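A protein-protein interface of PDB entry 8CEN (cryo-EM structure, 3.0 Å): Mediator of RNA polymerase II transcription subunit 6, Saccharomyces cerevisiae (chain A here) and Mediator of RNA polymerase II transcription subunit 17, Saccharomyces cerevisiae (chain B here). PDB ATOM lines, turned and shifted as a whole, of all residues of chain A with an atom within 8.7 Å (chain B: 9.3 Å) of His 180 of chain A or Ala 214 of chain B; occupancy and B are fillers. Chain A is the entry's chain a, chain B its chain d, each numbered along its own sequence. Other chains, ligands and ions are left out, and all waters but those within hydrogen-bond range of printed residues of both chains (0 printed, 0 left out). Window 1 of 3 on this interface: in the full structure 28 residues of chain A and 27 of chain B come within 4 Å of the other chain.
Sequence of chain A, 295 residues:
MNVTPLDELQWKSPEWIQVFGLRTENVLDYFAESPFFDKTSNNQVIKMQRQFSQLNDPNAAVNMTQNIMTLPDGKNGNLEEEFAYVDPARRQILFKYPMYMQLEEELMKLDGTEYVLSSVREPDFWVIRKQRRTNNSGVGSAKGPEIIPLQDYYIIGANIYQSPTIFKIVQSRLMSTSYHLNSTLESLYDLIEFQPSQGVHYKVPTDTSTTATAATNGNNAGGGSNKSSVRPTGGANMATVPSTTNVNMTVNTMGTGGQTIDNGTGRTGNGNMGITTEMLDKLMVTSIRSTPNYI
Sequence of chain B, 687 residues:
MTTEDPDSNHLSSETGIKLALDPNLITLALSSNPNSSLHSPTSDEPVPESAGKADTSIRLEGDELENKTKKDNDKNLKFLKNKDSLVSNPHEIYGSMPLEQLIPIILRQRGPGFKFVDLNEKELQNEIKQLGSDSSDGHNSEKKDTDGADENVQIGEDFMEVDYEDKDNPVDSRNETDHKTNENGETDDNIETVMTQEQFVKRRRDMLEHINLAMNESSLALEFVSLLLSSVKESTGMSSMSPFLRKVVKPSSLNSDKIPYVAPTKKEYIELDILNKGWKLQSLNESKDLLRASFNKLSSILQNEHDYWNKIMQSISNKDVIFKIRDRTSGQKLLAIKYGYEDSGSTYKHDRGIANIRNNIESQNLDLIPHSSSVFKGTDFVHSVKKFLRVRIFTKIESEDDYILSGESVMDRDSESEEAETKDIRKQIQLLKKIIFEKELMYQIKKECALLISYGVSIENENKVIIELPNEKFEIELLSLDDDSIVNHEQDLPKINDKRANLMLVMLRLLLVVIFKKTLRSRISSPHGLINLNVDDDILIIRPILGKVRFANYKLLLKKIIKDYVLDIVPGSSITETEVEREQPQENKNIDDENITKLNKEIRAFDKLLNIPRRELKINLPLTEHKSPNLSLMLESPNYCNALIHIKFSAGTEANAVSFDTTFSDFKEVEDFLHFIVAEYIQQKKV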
ATOM      1  N   SER A 172     -19.509  22.802 -13.002  1.00  0.00           N
ATOM      2  CA  SER A 172     -20.380  21.908 -12.242  1.00  0.00           C
ATOM      3  C   SER A 172     -19.749  20.533 -12.072  1.00  0.00           C
ATOM      4  O   SER A 172     -19.824  19.934 -10.986  1.00  0.00           O
ATOM      5  CB  SER A 172     -21.733  21.786 -12.938  1.00  0.00           C
ATOM      6  OG  SER A 172     -21.590  21.199 -14.218  1.00  0.00           O
ATOM      7  N   ARG A 173     -19.115  20.021 -13.133  1.00  0.00           N
ATOM      8  CA  ARG A 173     -18.431  18.734 -13.031  1.00  0.00           C
ATOM      9  C   ARG A 173     -17.292  18.787 -12.019  1.00  0.00           C
ATOM     10  O   ARG A 173     -17.084  17.838 -11.254  1.00  0.00           O
ATOM     11  CB  ARG A 173     -17.908  18.310 -14.398  1.00  0.00           C
ATOM     12  CG  ARG A 173     -18.969  17.921 -15.411  1.00  0.00           C
ATOM     13  CD  ARG A 173     -19.856  16.805 -14.893  1.00  0.00           C
ATOM     14  NE  ARG A 173     -20.717  16.277 -15.943  1.00  0.00           N
ATOM     15  CZ  ARG A 173     -21.624  15.327 -15.763  1.00  0.00           C
ATOM     16  NH1 ARG A 173     -21.833  14.787 -14.574  1.00  0.00           N
ATOM     17  NH2 ARG A 173     -22.336  14.905 -16.804  1.00  0.00           N
ATOM     18  N   LEU A 174     -16.557  19.900 -11.978  1.00  0.00           N
ATOM     19  CA  LEU A 174     -15.468  20.027 -11.019  1.00  0.00           C
ATOM     20  C   LEU A 174     -15.963  20.311  -9.602  1.00  0.00           C
ATOM     21  O   LEU A 174     -15.278  19.948  -8.645  1.00  0.00           O
ATOM     22  CB  LEU A 174     -14.490  21.104 -11.487  1.00  0.00           C
ATOM     23  CG  LEU A 174     -13.586  20.663 -12.642  1.00  0.00           C
ATOM     24  CD1 LEU A 174     -12.817  21.836 -13.226  1.00  0.00           C
ATOM     25  CD2 LEU A 174     -12.633  19.569 -12.185  1.00  0.00           C
ATOM     26  N   MET A 175     -17.135  20.936  -9.439  1.00  0.00           N
ATOM     27  CA  MET A 175     -17.778  20.984  -8.124  1.00  0.00           C
ATOM     28  C   MET A 175     -18.090  19.588  -7.614  1.00  0.00           C
ATOM     29  O   MET A 175     -17.835  19.270  -6.446  1.00  0.00           O
ATOM     30  CB  MET A 175     -19.064  21.816  -8.165  1.00  0.00           C
ATOM     31  CG  MET A 175     -18.897  23.291  -8.425  1.00  0.00           C
ATOM     32  SD  MET A 175     -17.919  24.036  -7.122  1.00  0.00           S
ATOM     33  CE  MET A 175     -19.074  23.915  -5.763  1.00  0.00           C
ATOM     34  N   SER A 176     -18.655  18.742  -8.480  1.00  0.00           N
ATOM     35  CA  SER A 176     -18.940  17.366  -8.080  1.00  0.00           C
ATOM     36  C   SER A 176     -17.655  16.610  -7.757  1.00  0.00           C
ATOM     37  O   SER A 176     -17.589  15.875  -6.761  1.00  0.00           O
ATOM     38  CB  SER A 176     -19.725  16.657  -9.180  1.00  0.00           C
ATOM     39  OG  SER A 176     -20.961  17.301  -9.425  1.00  0.00           O
ATOM     40  N   THR A 177     -16.618  16.805  -8.578  1.00  0.00           N
ATOM     41  CA  THR A 177     -15.327  16.163  -8.347  1.00  0.00           C
ATOM     42  C   THR A 177     -14.718  16.602  -7.021  1.00  0.00           C
ATOM     43  O   THR A 177     -14.225  15.774  -6.248  1.00  0.00           O
ATOM     44  CB  THR A 177     -14.378  16.482  -9.505  1.00  0.00           C
ATOM     45  OG1 THR A 177     -14.937  15.996 -10.731  1.00  0.00           O
ATOM     46  CG2 THR A 177     -13.018  15.835  -9.288  1.00  0.00           C
ATOM     47  N   SER A 178     -14.767  17.906  -6.731  1.00  0.00           N
ATOM     48  CA  SER A 178     -14.195  18.429  -5.496  1.00  0.00           C
ATOM     49  C   SER A 178     -14.970  17.956  -4.274  1.00  0.00           C
ATOM     50  O   SER A 178     -14.367  17.636  -3.245  1.00  0.00           O
ATOM     51  CB  SER A 178     -14.149  19.955  -5.547  1.00  0.00           C
ATOM     52  OG  SER A 178     -13.906  20.501  -4.263  1.00  0.00           O
ATOM     53  N   TYR A 179     -16.303  17.897  -4.368  1.00  0.00           N
ATOM     54  CA  TYR A 179     -17.105  17.417  -3.244  1.00  0.00           C
ATOM     55  C   TYR A 179     -16.819  15.948  -2.955  1.00  0.00           C
ATOM     56  O   TYR A 179     -16.629  15.556  -1.794  1.00  0.00           O
ATOM     57  CB  TYR A 179     -18.594  17.658  -3.529  1.00  0.00           C
ATOM     58  CG  TYR A 179     -19.574  16.959  -2.598  1.00  0.00           C
ATOM     59  CD1 TYR A 179     -20.049  15.676  -2.871  1.00  0.00           C
ATOM     60  CD2 TYR A 179     -20.015  17.581  -1.437  1.00  0.00           C
ATOM     61  CE1 TYR A 179     -20.932  15.044  -2.018  1.00  0.00           C
ATOM     62  CE2 TYR A 179     -20.900  16.954  -0.580  1.00  0.00           C
ATOM     63  CZ  TYR A 179     -21.354  15.686  -0.876  1.00  0.00           C
ATOM     64  OH  TYR A 179     -22.234  15.058  -0.026  1.00  0.00           O
ATOM     65  N   HIS A 180     -16.771  15.119  -4.003  1.00  0.00           N
ATOM     66  CA  HIS A 180     -16.514  13.698  -3.800  1.00  0.00           C
ATOM     67  C   HIS A 180     -15.086  13.456  -3.323  1.00  0.00           C
ATOM     68  O   HIS A 180     -14.847  12.579  -2.484  1.00  0.00           O
ATOM     69  CB  HIS A 180     -16.805  12.929  -5.087  1.00  0.00           C
ATOM     70  CG  HIS A 180     -18.260  12.867  -5.433  1.00  0.00           C
ATOM     71  ND1 HIS A 180     -19.228  12.525  -4.514  1.00  0.00           N
ATOM     72  CD2 HIS A 180     -18.913  13.112  -6.594  1.00  0.00           C
ATOM     73  CE1 HIS A 180     -20.415  12.559  -5.094  1.00  0.00           C
ATOM     74  NE2 HIS A 180     -20.251  12.912  -6.357  1.00  0.00           N
ATOM     75  N   LEU A 181     -14.130  14.246  -3.819  1.00  0.00           N
ATOM     76  CA  LEU A 181     -12.751  14.135  -3.361  1.00  0.00           C
ATOM     77  C   LEU A 181     -12.609  14.558  -1.905  1.00  0.00           C
ATOM     78  O   LEU A 181     -11.860  13.933  -1.149  1.00  0.00           O
ATOM     79  CB  LEU A 181     -11.839  14.970  -4.259  1.00  0.00           C
ATOM     80  CG  LEU A 181     -10.335  14.734  -4.125  1.00  0.00           C
ATOM     81  CD1 LEU A 181     -10.000  13.270  -4.339  1.00  0.00           C
ATOM     82  CD2 LEU A 181      -9.582  15.603  -5.115  1.00  0.00           C
ATOM     83  N   ASN A 182     -13.321  15.611  -1.492  1.00  0.00           N
ATOM     84  CA  ASN A 182     -13.273  16.042  -0.099  1.00  0.00           C
ATOM     85  C   ASN A 182     -13.898  15.003   0.824  1.00  0.00           C
ATOM     86  O   ASN A 182     -13.390  14.760   1.927  1.00  0.00           O
ATOM     87  CB  ASN A 182     -13.975  17.391   0.053  1.00  0.00           C
ATOM     88  CG  ASN A 182     -14.094  17.828   1.499  1.00  0.00           C
ATOM     89  OD1 ASN A 182     -13.122  18.276   2.106  1.00  0.00           O
ATOM     90  ND2 ASN A 182     -15.291  17.702   2.058  1.00  0.00           N
ATOM     91  N   SER A 183     -14.996  14.378   0.386  1.00  0.00           N
ATOM     92  CA  SER A 183     -15.590  13.297   1.169  1.00  0.00           C
ATOM     93  C   SER A 183     -14.644  12.106   1.279  1.00  0.00           C
ATOM     94  O   SER A 183     -14.514  11.505   2.355  1.00  0.00           O
ATOM     95  CB  SER A 183     -16.922  12.873   0.549  1.00  0.00           C
ATOM     96  OG  SER A 183     -17.871  13.922   0.620  1.00  0.00           O
ATOM     97  N   THR A 184     -13.965  11.764   0.175  1.00  0.00           N
ATOM     98  CA  THR A 184     -12.973  10.691   0.193  1.00  0.00           C
ATOM     99  C   THR A 184     -11.834  11.012   1.152  1.00  0.00           C
ATOM    100  O   THR A 184     -11.410  10.151   1.933  1.00  0.00           O
ATOM    101  CB  THR A 184     -12.423  10.466  -1.218  1.00  0.00           C
ATOM    102  OG1 THR A 184     -13.489  10.103  -2.100  1.00  0.00           O
ATOM    103  CG2 THR A 184     -11.380   9.356  -1.224  1.00  0.00           C
ATOM    104  N   LEU A 185     -11.351  12.257   1.122  1.00  0.00           N
ATOM    105  CA  LEU A 185     -10.263  12.675   1.999  1.00  0.00           C
ATOM    106  C   LEU A 185     -10.670  12.604   3.465  1.00  0.00           C
ATOM    107  O   LEU A 185      -9.918  12.087   4.294  1.00  0.00           O
ATOM    108  CB  LEU A 185      -9.809  14.088   1.631  1.00  0.00           C
ATOM    109  CG  LEU A 185      -9.002  14.212   0.336  1.00  0.00           C
ATOM    110  CD1 LEU A 185      -8.846  15.659  -0.085  1.00  0.00           C
ATOM    111  CD2 LEU A 185      -7.646  13.579   0.523  1.00  0.00           C
ATOM    112  N   GLU A 186     -11.867  13.095   3.800  1.00  0.00           N
ATOM    113  CA  GLU A 186     -12.299  13.096   5.197  1.00  0.00           C
ATOM    114  C   GLU A 186     -12.529  11.677   5.711  1.00  0.00           C
ATOM    115  O   GLU A 186     -12.109  11.335   6.827  1.00  0.00           O
ATOM    116  CB  GLU A 186     -13.558  13.958   5.343  1.00  0.00           C
ATOM    117  CG  GLU A 186     -14.010  14.255   6.778  1.00  0.00           C
ATOM    118  CD  GLU A 186     -14.857  13.151   7.386  1.00  0.00           C
ATOM    119  OE1 GLU A 186     -15.548  12.447   6.620  1.00  0.00           O
ATOM    120  OE2 GLU A 186     -14.823  12.979   8.622  1.00  0.00           O
ATOM    121  N   SER A 187     -13.164  10.828   4.901  1.00  0.00           N
ATOM    122  CA  SER A 187     -13.377   9.444   5.304  1.00  0.00           C
ATOM    123  C   SER A 187     -12.072   8.655   5.378  1.00  0.00           C
ATOM    124  O   SER A 187     -11.974   7.705   6.163  1.00  0.00           O
ATOM    125  CB  SER A 187     -14.367   8.790   4.347  1.00  0.00           C
ATOM    126  OG  SER A 187     -13.864   8.846   3.032  1.00  0.00           O
ATOM    127  N   ASP B 206     -17.521   3.275   1.345  1.00  0.00           N
ATOM    128  CA  ASP B 206     -18.062   4.582   0.993  1.00  0.00           C
ATOM    129  C   ASP B 206     -16.990   5.506   0.422  1.00  0.00           C
ATOM    130  O   ASP B 206     -17.282   6.292  -0.487  1.00  0.00           O
ATOM    131  CB  ASP B 206     -18.820   5.204   2.185  1.00  0.00           C
ATOM    132  CG  ASP B 206     -17.935   5.572   3.386  1.00  0.00           C
ATOM    133  OD1 ASP B 206     -16.836   6.148   3.247  1.00  0.00           O
ATOM    134  OD2 ASP B 206     -18.381   5.292   4.517  1.00  0.00           O
ATOM    135  N   MET B 207     -15.739   5.404   0.888  1.00  0.00           N
ATOM    136  CA  MET B 207     -14.714   6.225   0.250  1.00  0.00           C
ATOM    137  C   MET B 207     -14.347   5.683  -1.125  1.00  0.00           C
ATOM    138  O   MET B 207     -14.004   6.467  -2.021  1.00  0.00           O
ATOM    139  CB  MET B 207     -13.480   6.370   1.143  1.00  0.00           C
ATOM    140  CG  MET B 207     -12.650   5.151   1.449  1.00  0.00           C
ATOM    141  SD  MET B 207     -11.339   5.698   2.565  1.00  0.00           S
ATOM    142  CE  MET B 207     -10.444   4.183   2.856  1.00  0.00           C
ATOM    143  N   LEU B 208     -14.461   4.365  -1.332  1.00  0.00           N
ATOM    144  CA  LEU B 208     -14.302   3.811  -2.673  1.00  0.00           C
ATOM    145  C   LEU B 208     -15.377   4.329  -3.625  1.00  0.00           C
ATOM    146  O   LEU B 208     -15.076   4.701  -4.765  1.00  0.00           O
ATOM    147  CB  LEU B 208     -14.323   2.283  -2.612  1.00  0.00           C
ATOM    148  CG  LEU B 208     -14.519   1.525  -3.928  1.00  0.00           C
ATOM    149  CD1 LEU B 208     -13.339   1.739  -4.856  1.00  0.00           C
ATOM    150  CD2 LEU B 208     -14.729   0.039  -3.659  1.00  0.00           C
ATOM    151  N   GLU B 209     -16.631   4.392  -3.172  1.00  0.00           N
ATOM    152  CA  GLU B 209     -17.672   4.877  -4.074  1.00  0.00           C
ATOM    153  C   GLU B 209     -17.574   6.386  -4.285  1.00  0.00           C
ATOM    154  O   GLU B 209     -17.895   6.876  -5.375  1.00  0.00           O
ATOM    155  CB  GLU B 209     -19.065   4.468  -3.578  1.00  0.00           C
ATOM    156  CG  GLU B 209     -19.652   5.280  -2.438  1.00  0.00           C
ATOM    157  CD  GLU B 209     -21.073   4.865  -2.107  1.00  0.00           C
ATOM    158  OE1 GLU B 209     -21.572   3.902  -2.728  1.00  0.00           O
ATOM    159  OE2 GLU B 209     -21.695   5.506  -1.234  1.00  0.00           O
ATOM    160  N   HIS B 210     -17.091   7.136  -3.286  1.00  0.00           N
ATOM    161  CA  HIS B 210     -16.881   8.567  -3.486  1.00  0.00           C
ATOM    162  C   HIS B 210     -15.745   8.836  -4.468  1.00  0.00           C
ATOM    163  O   HIS B 210     -15.842   9.749  -5.299  1.00  0.00           O
ATOM    164  CB  HIS B 210     -16.619   9.261  -2.150  1.00  0.00           C
ATOM    165  CG  HIS B 210     -17.835   9.396  -1.288  1.00  0.00           C
ATOM    166  ND1 HIS B 210     -18.204   8.444  -0.364  1.00  0.00           N
ATOM    167  CD2 HIS B 210     -18.769  10.374  -1.214  1.00  0.00           C
ATOM    168  CE1 HIS B 210     -19.312   8.829   0.245  1.00  0.00           C
ATOM    169  NE2 HIS B 210     -19.675   9.997  -0.253  1.00  0.00           N
ATOM    170  N   ILE B 211     -14.663   8.051  -4.404  1.00  0.00           N
ATOM    171  CA  ILE B 211     -13.591   8.247  -5.375  1.00  0.00           C
ATOM    172  C   ILE B 211     -14.028   7.775  -6.761  1.00  0.00           C
ATOM    173  O   ILE B 211     -13.600   8.343  -7.777  1.00  0.00           O
ATOM    174  CB  ILE B 211     -12.278   7.583  -4.897  1.00  0.00           C
ATOM    175  CG1 ILE B 211     -11.076   8.294  -5.514  1.00  0.00           C
ATOM    176  CG2 ILE B 211     -12.204   6.101  -5.225  1.00  0.00           C
ATOM    177  CD1 ILE B 211     -10.991   9.750  -5.150  1.00  0.00           C
ATOM    178  N   ASN B 212     -14.919   6.774  -6.831  1.00  0.00           N
ATOM    179  CA  ASN B 212     -15.499   6.381  -8.113  1.00  0.00           C
ATOM    180  C   ASN B 212     -16.321   7.511  -8.716  1.00  0.00           C
ATOM    181  O   ASN B 212     -16.219   7.792  -9.915  1.00  0.00           O
ATOM    182  CB  ASN B 212     -16.371   5.137  -7.942  1.00  0.00           C
ATOM    183  CG  ASN B 212     -15.561   3.875  -7.745  1.00  0.00           C
ATOM    184  OD1 ASN B 212     -14.447   3.756  -8.246  1.00  0.00           O
ATOM    185  ND2 ASN B 212     -16.121   2.921  -7.011  1.00  0.00           N
ATOM    186  N   LEU B 213     -17.135   8.176  -7.892  1.00  0.00           N
ATOM    187  CA  LEU B 213     -17.946   9.286  -8.382  1.00  0.00           C
ATOM    188  C   LEU B 213     -17.081  10.467  -8.808  1.00  0.00           C
ATOM    189  O   LEU B 213     -17.374  11.120  -9.820  1.00  0.00           O
ATOM    190  CB  LEU B 213     -18.954   9.706  -7.314  1.00  0.00           C
ATOM    191  CG  LEU B 213     -20.075   8.704  -7.033  1.00  0.00           C
ATOM    192  CD1 LEU B 213     -20.871   9.114  -5.806  1.00  0.00           C
ATOM    193  CD2 LEU B 213     -20.982   8.561  -8.245  1.00  0.00           C
ATOM    194  N   ALA B 214     -16.011  10.752  -8.056  1.00  0.00           N
ATOM    195  CA  ALA B 214     -15.097  11.830  -8.433  1.00  0.00           C
ATOM    196  C   ALA B 214     -14.413  11.542  -9.764  1.00  0.00           C
ATOM    197  O   ALA B 214     -14.323  12.427 -10.629  1.00  0.00           O
ATOM    198  CB  ALA B 214     -14.053  12.042  -7.339  1.00  0.00           C
ATOM    199  N   MET B 215     -13.936  10.306  -9.947  1.00  0.00           N
ATOM    200  CA  MET B 215     -13.330   9.917 -11.216  1.00  0.00           C
ATOM    201  C   MET B 215     -14.333  10.004 -12.358  1.00  0.00           C
ATOM    202  O   MET B 215     -13.993  10.457 -13.456  1.00  0.00           O
ATOM    203  CB  MET B 215     -12.778   8.498 -11.122  1.00  0.00           C
ATOM    204  CG  MET B 215     -12.083   8.041 -12.385  1.00  0.00           C
ATOM    205  SD  MET B 215     -11.631   6.311 -12.289  1.00  0.00           S
ATOM    206  CE  MET B 215     -13.245   5.611 -12.612  1.00  0.00           C
ATOM    207  N   ASN B 216     -15.575   9.572 -12.112  1.00  0.00           N
ATOM    208  CA  ASN B 216     -16.607   9.611 -13.144  1.00  0.00           C
ATOM    209  C   ASN B 216     -16.914  11.039 -13.577  1.00  0.00           C
ATOM    210  O   ASN B 216     -17.020  11.322 -14.776  1.00  0.00           O
ATOM    211  CB  ASN B 216     -17.873   8.926 -12.636  1.00  0.00           C
ATOM    212  CG  ASN B 216     -18.706   8.341 -13.753  1.00  0.00           C
ATOM    213  OD1 ASN B 216     -18.245   8.210 -14.886  1.00  0.00           O
ATOM    214  ND2 ASN B 216     -19.947   7.992 -13.441  1.00  0.00           N
ATOM    215  N   GLU B 217     -17.037  11.956 -12.614  1.00  0.00           N
ATOM    216  CA  GLU B 217     -17.338  13.344 -12.951  1.00  0.00           C
ATOM    217  C   GLU B 217     -16.171  14.011 -13.673  1.00  0.00           C
ATOM    218  O   GLU B 217     -16.377  14.746 -14.652  1.00  0.00           O
ATOM    219  CB  GLU B 217     -17.708  14.115 -11.686  1.00  0.00           C
ATOM    220  CG  GLU B 217     -19.010  13.647 -11.058  1.00  0.00           C
ATOM    221  CD  GLU B 217     -20.198  13.807 -11.984  1.00  0.00           C
ATOM    222  OE1 GLU B 217     -20.635  14.955 -12.204  1.00  0.00           O
ATOM    223  OE2 GLU B 217     -20.696  12.781 -12.496  1.00  0.00           O
ATOM    224  N   SER B 218     -14.939  13.749 -13.219  1.00  0.00           N
ATOM    225  CA  SER B 218     -13.770  14.312 -13.886  1.00  0.00           C
ATOM    226  C   SER B 218     -13.626  13.774 -15.305  1.00  0.00           C
ATOM    227  O   SER B 218     -13.285  14.524 -16.229  1.00  0.00           O
ATOM    228  CB  SER B 218     -12.512  14.021 -13.071  1.00  0.00           C
ATOM    229  OG  SER B 218     -11.345  14.397 -13.782  1.00  0.00           O
ATOM    230  N   SER B 219     -13.904  12.483 -15.504  1.00  0.00           N
ATOM    231  CA  SER B 219     -13.817  11.904 -16.840  1.00  0.00           C
ATOM    232  C   SER B 219     -14.917  12.435 -17.748  1.00  0.00           C
ATOM    233  O   SER B 219     -14.681  12.651 -18.941  1.00  0.00           O
ATOM    234  CB  SER B 219     -13.875  10.381 -16.764  1.00  0.00           C
ATOM    235  OG  SER B 219     -14.933   9.953 -15.931  1.00  0.00           O
ATOM    236  N   LEU B 220     -16.122  12.648 -17.211  1.00  0.00           N
ATOM    237  CA  LEU B 220     -17.194  13.232 -18.012  1.00  0.00           C
ATOM    238  C   LEU B 220     -16.841  14.645 -18.460  1.00  0.00           C
ATOM    239  O   LEU B 220     -17.073  15.013 -19.620  1.00  0.00           O
ATOM    240  CB  LEU B 220     -18.503  13.229 -17.224  1.00  0.00           C
ATOM    241  CG  LEU B 220     -19.277  11.910 -17.212  1.00  0.00           C
ATOM    242  CD1 LEU B 220     -20.460  11.989 -16.263  1.00  0.00           C
ATOM    243  CD2 LEU B 220     -19.735  11.551 -18.615  1.00  0.00           C
ATOM    244  N   ALA B 221     -16.253  15.441 -17.560  1.00  0.00           N
ATOM    245  CA  ALA B 221     -15.792  16.775 -17.939  1.00  0.00           C
ATOM    246  C   ALA B 221     -14.696  16.708 -18.996  1.00  0.00           C
ATOM    247  O   ALA B 221     -14.728  17.460 -19.981  1.00  0.00           O
ATOM    248  CB  ALA B 221     -15.289  17.523 -16.709  1.00  0.00           C
ATOM    249  N   LEU B 222     -13.729  15.801 -18.812  1.00  0.00           N
ATOM    250  CA  LEU B 222     -12.632  15.648 -19.762  1.00  0.00           C
ATOM    251  C   LEU B 222     -13.139  15.254 -21.140  1.00  0.00           C
ATOM    252  O   LEU B 222     -12.665  15.772 -22.157  1.00  0.00           O
ATOM    253  CB  LEU B 222     -11.643  14.601 -19.247  1.00  0.00           C
ATOM    254  CG  LEU B 222     -10.568  14.132 -20.229  1.00  0.00           C
ATOM    255  CD1 LEU B 222      -9.645  15.275 -20.612  1.00  0.00           C
ATOM    256  CD2 LEU B 222      -9.788  12.957 -19.663  1.00  0.00           C
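Of the 16 printed residues of chain A, 8 touch a printed residue of chain B.
Along chain A the printed residues that touch a printed residue of chain B span positions 173 to 187.
Of the 17 printed residues of chain B, 10 touch a printed residue of chain A.
Among the printed residues, 17 pairs touch across the chains.
Of the printed residues of chain B, Thr 177 of chain A touches Ala 214, Glu 217 and Ser 218.
Tyr 179 of chain A touches none of the printed residues of chain B.
Of chain B, only His 210 (3.3 Å), Leu 213 (3.5 Å) and Ala 214 (3.7 Å) come within 4 Å of His 180 of chain A.
Printed residues of chain B within 4 Å of Thr 184 of chain A: Met 207, His 210 and Ile 211.
Of the printed residues of chain A, Met 207 of chain B touches Thr 184 and Ser 187.
Ala 214 of chain B touches just these residues of chain A: Thr 177 and His 180.
The nearest residue of chain A that does not touch Ala 214 of chain B is Leu 181 of chain A (4.2 Å).
The nearest printed residue of chain A that does not touch Ile 211 of chain B is His 180 of chain A (4.9 Å).
Among the printed residues, pairs that only touch across the chains: Arg 173 of chain A with Leu 220 of chain B, Arg 173 of chain A with Ala 221 of chain B, Ser 176 of chain A with Glu 217 of chain B, Thr 177 of chain A with Ala 214 of chain B, Thr 177 of chain A with Glu 217 of chain B, His 180 of chain A with His 210 of chain B, His 180 of chain A with Leu 213 of chain B, His 180 of chain A with Ala 214 of chain B, Leu 181 of chain A with Ile 211 of chain B, Ser 183 of chain A with His 210 of chain B, Thr 184 of chain A with Met 207 of chain B, Thr 184 of chain A with His 210 of chain B, Ser 187 of chain A with Asp 206 of chain B and Ser 187 of chain A with Met 207 of chain B.
The guanidinium group (NH1) of Arg 173 of chain A is in salt-bridge range of the side-chain carboxylate (OE1) of Glu 217 of chain B, at 2.7 Å.
The side-chain hydroxyl (OG1) of Thr 177 of chain A sits at hydrogen-bond distance from the backbone NH (N) of Ser 218 of chain B, at 3.4 Å.
N of Ile 211 of chain B lies within hydrogen-bond range of OG1 of Thr 184 of chain A.
The backbone carbonyl oxygen (O) of Ser 172 of chain A lies within hydrogen-bond range of the side-chain hydroxyl (OG) of Ser 176 of chain A.
The backbone carbonyl oxygen (O) of Arg 173 of chain A is in hydrogen-bond range of the side-chain hydroxyl (OG1) of Thr 177 of chain A, at 2.9 Å.
O of Tyr 179 of chain A lies within hydrogen-bond range of OG of Ser 183 of chain A.
The side-chain hydroxyl of Thr 184 of chain A sits at hydrogen-bond distance from the backbone carbonyl oxygen of His 180 of chain A, at 2.8 Å.
The backbone carbonyl oxygen (O) of Ser 183 of chain A sits at hydrogen-bond distance from the side-chain hydroxyl (OG) of Ser 187 of chain A.
OG of Ser 187 of chain A lies within hydrogen-bond range of O of Thr 184 of chain A (3.0 Å).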
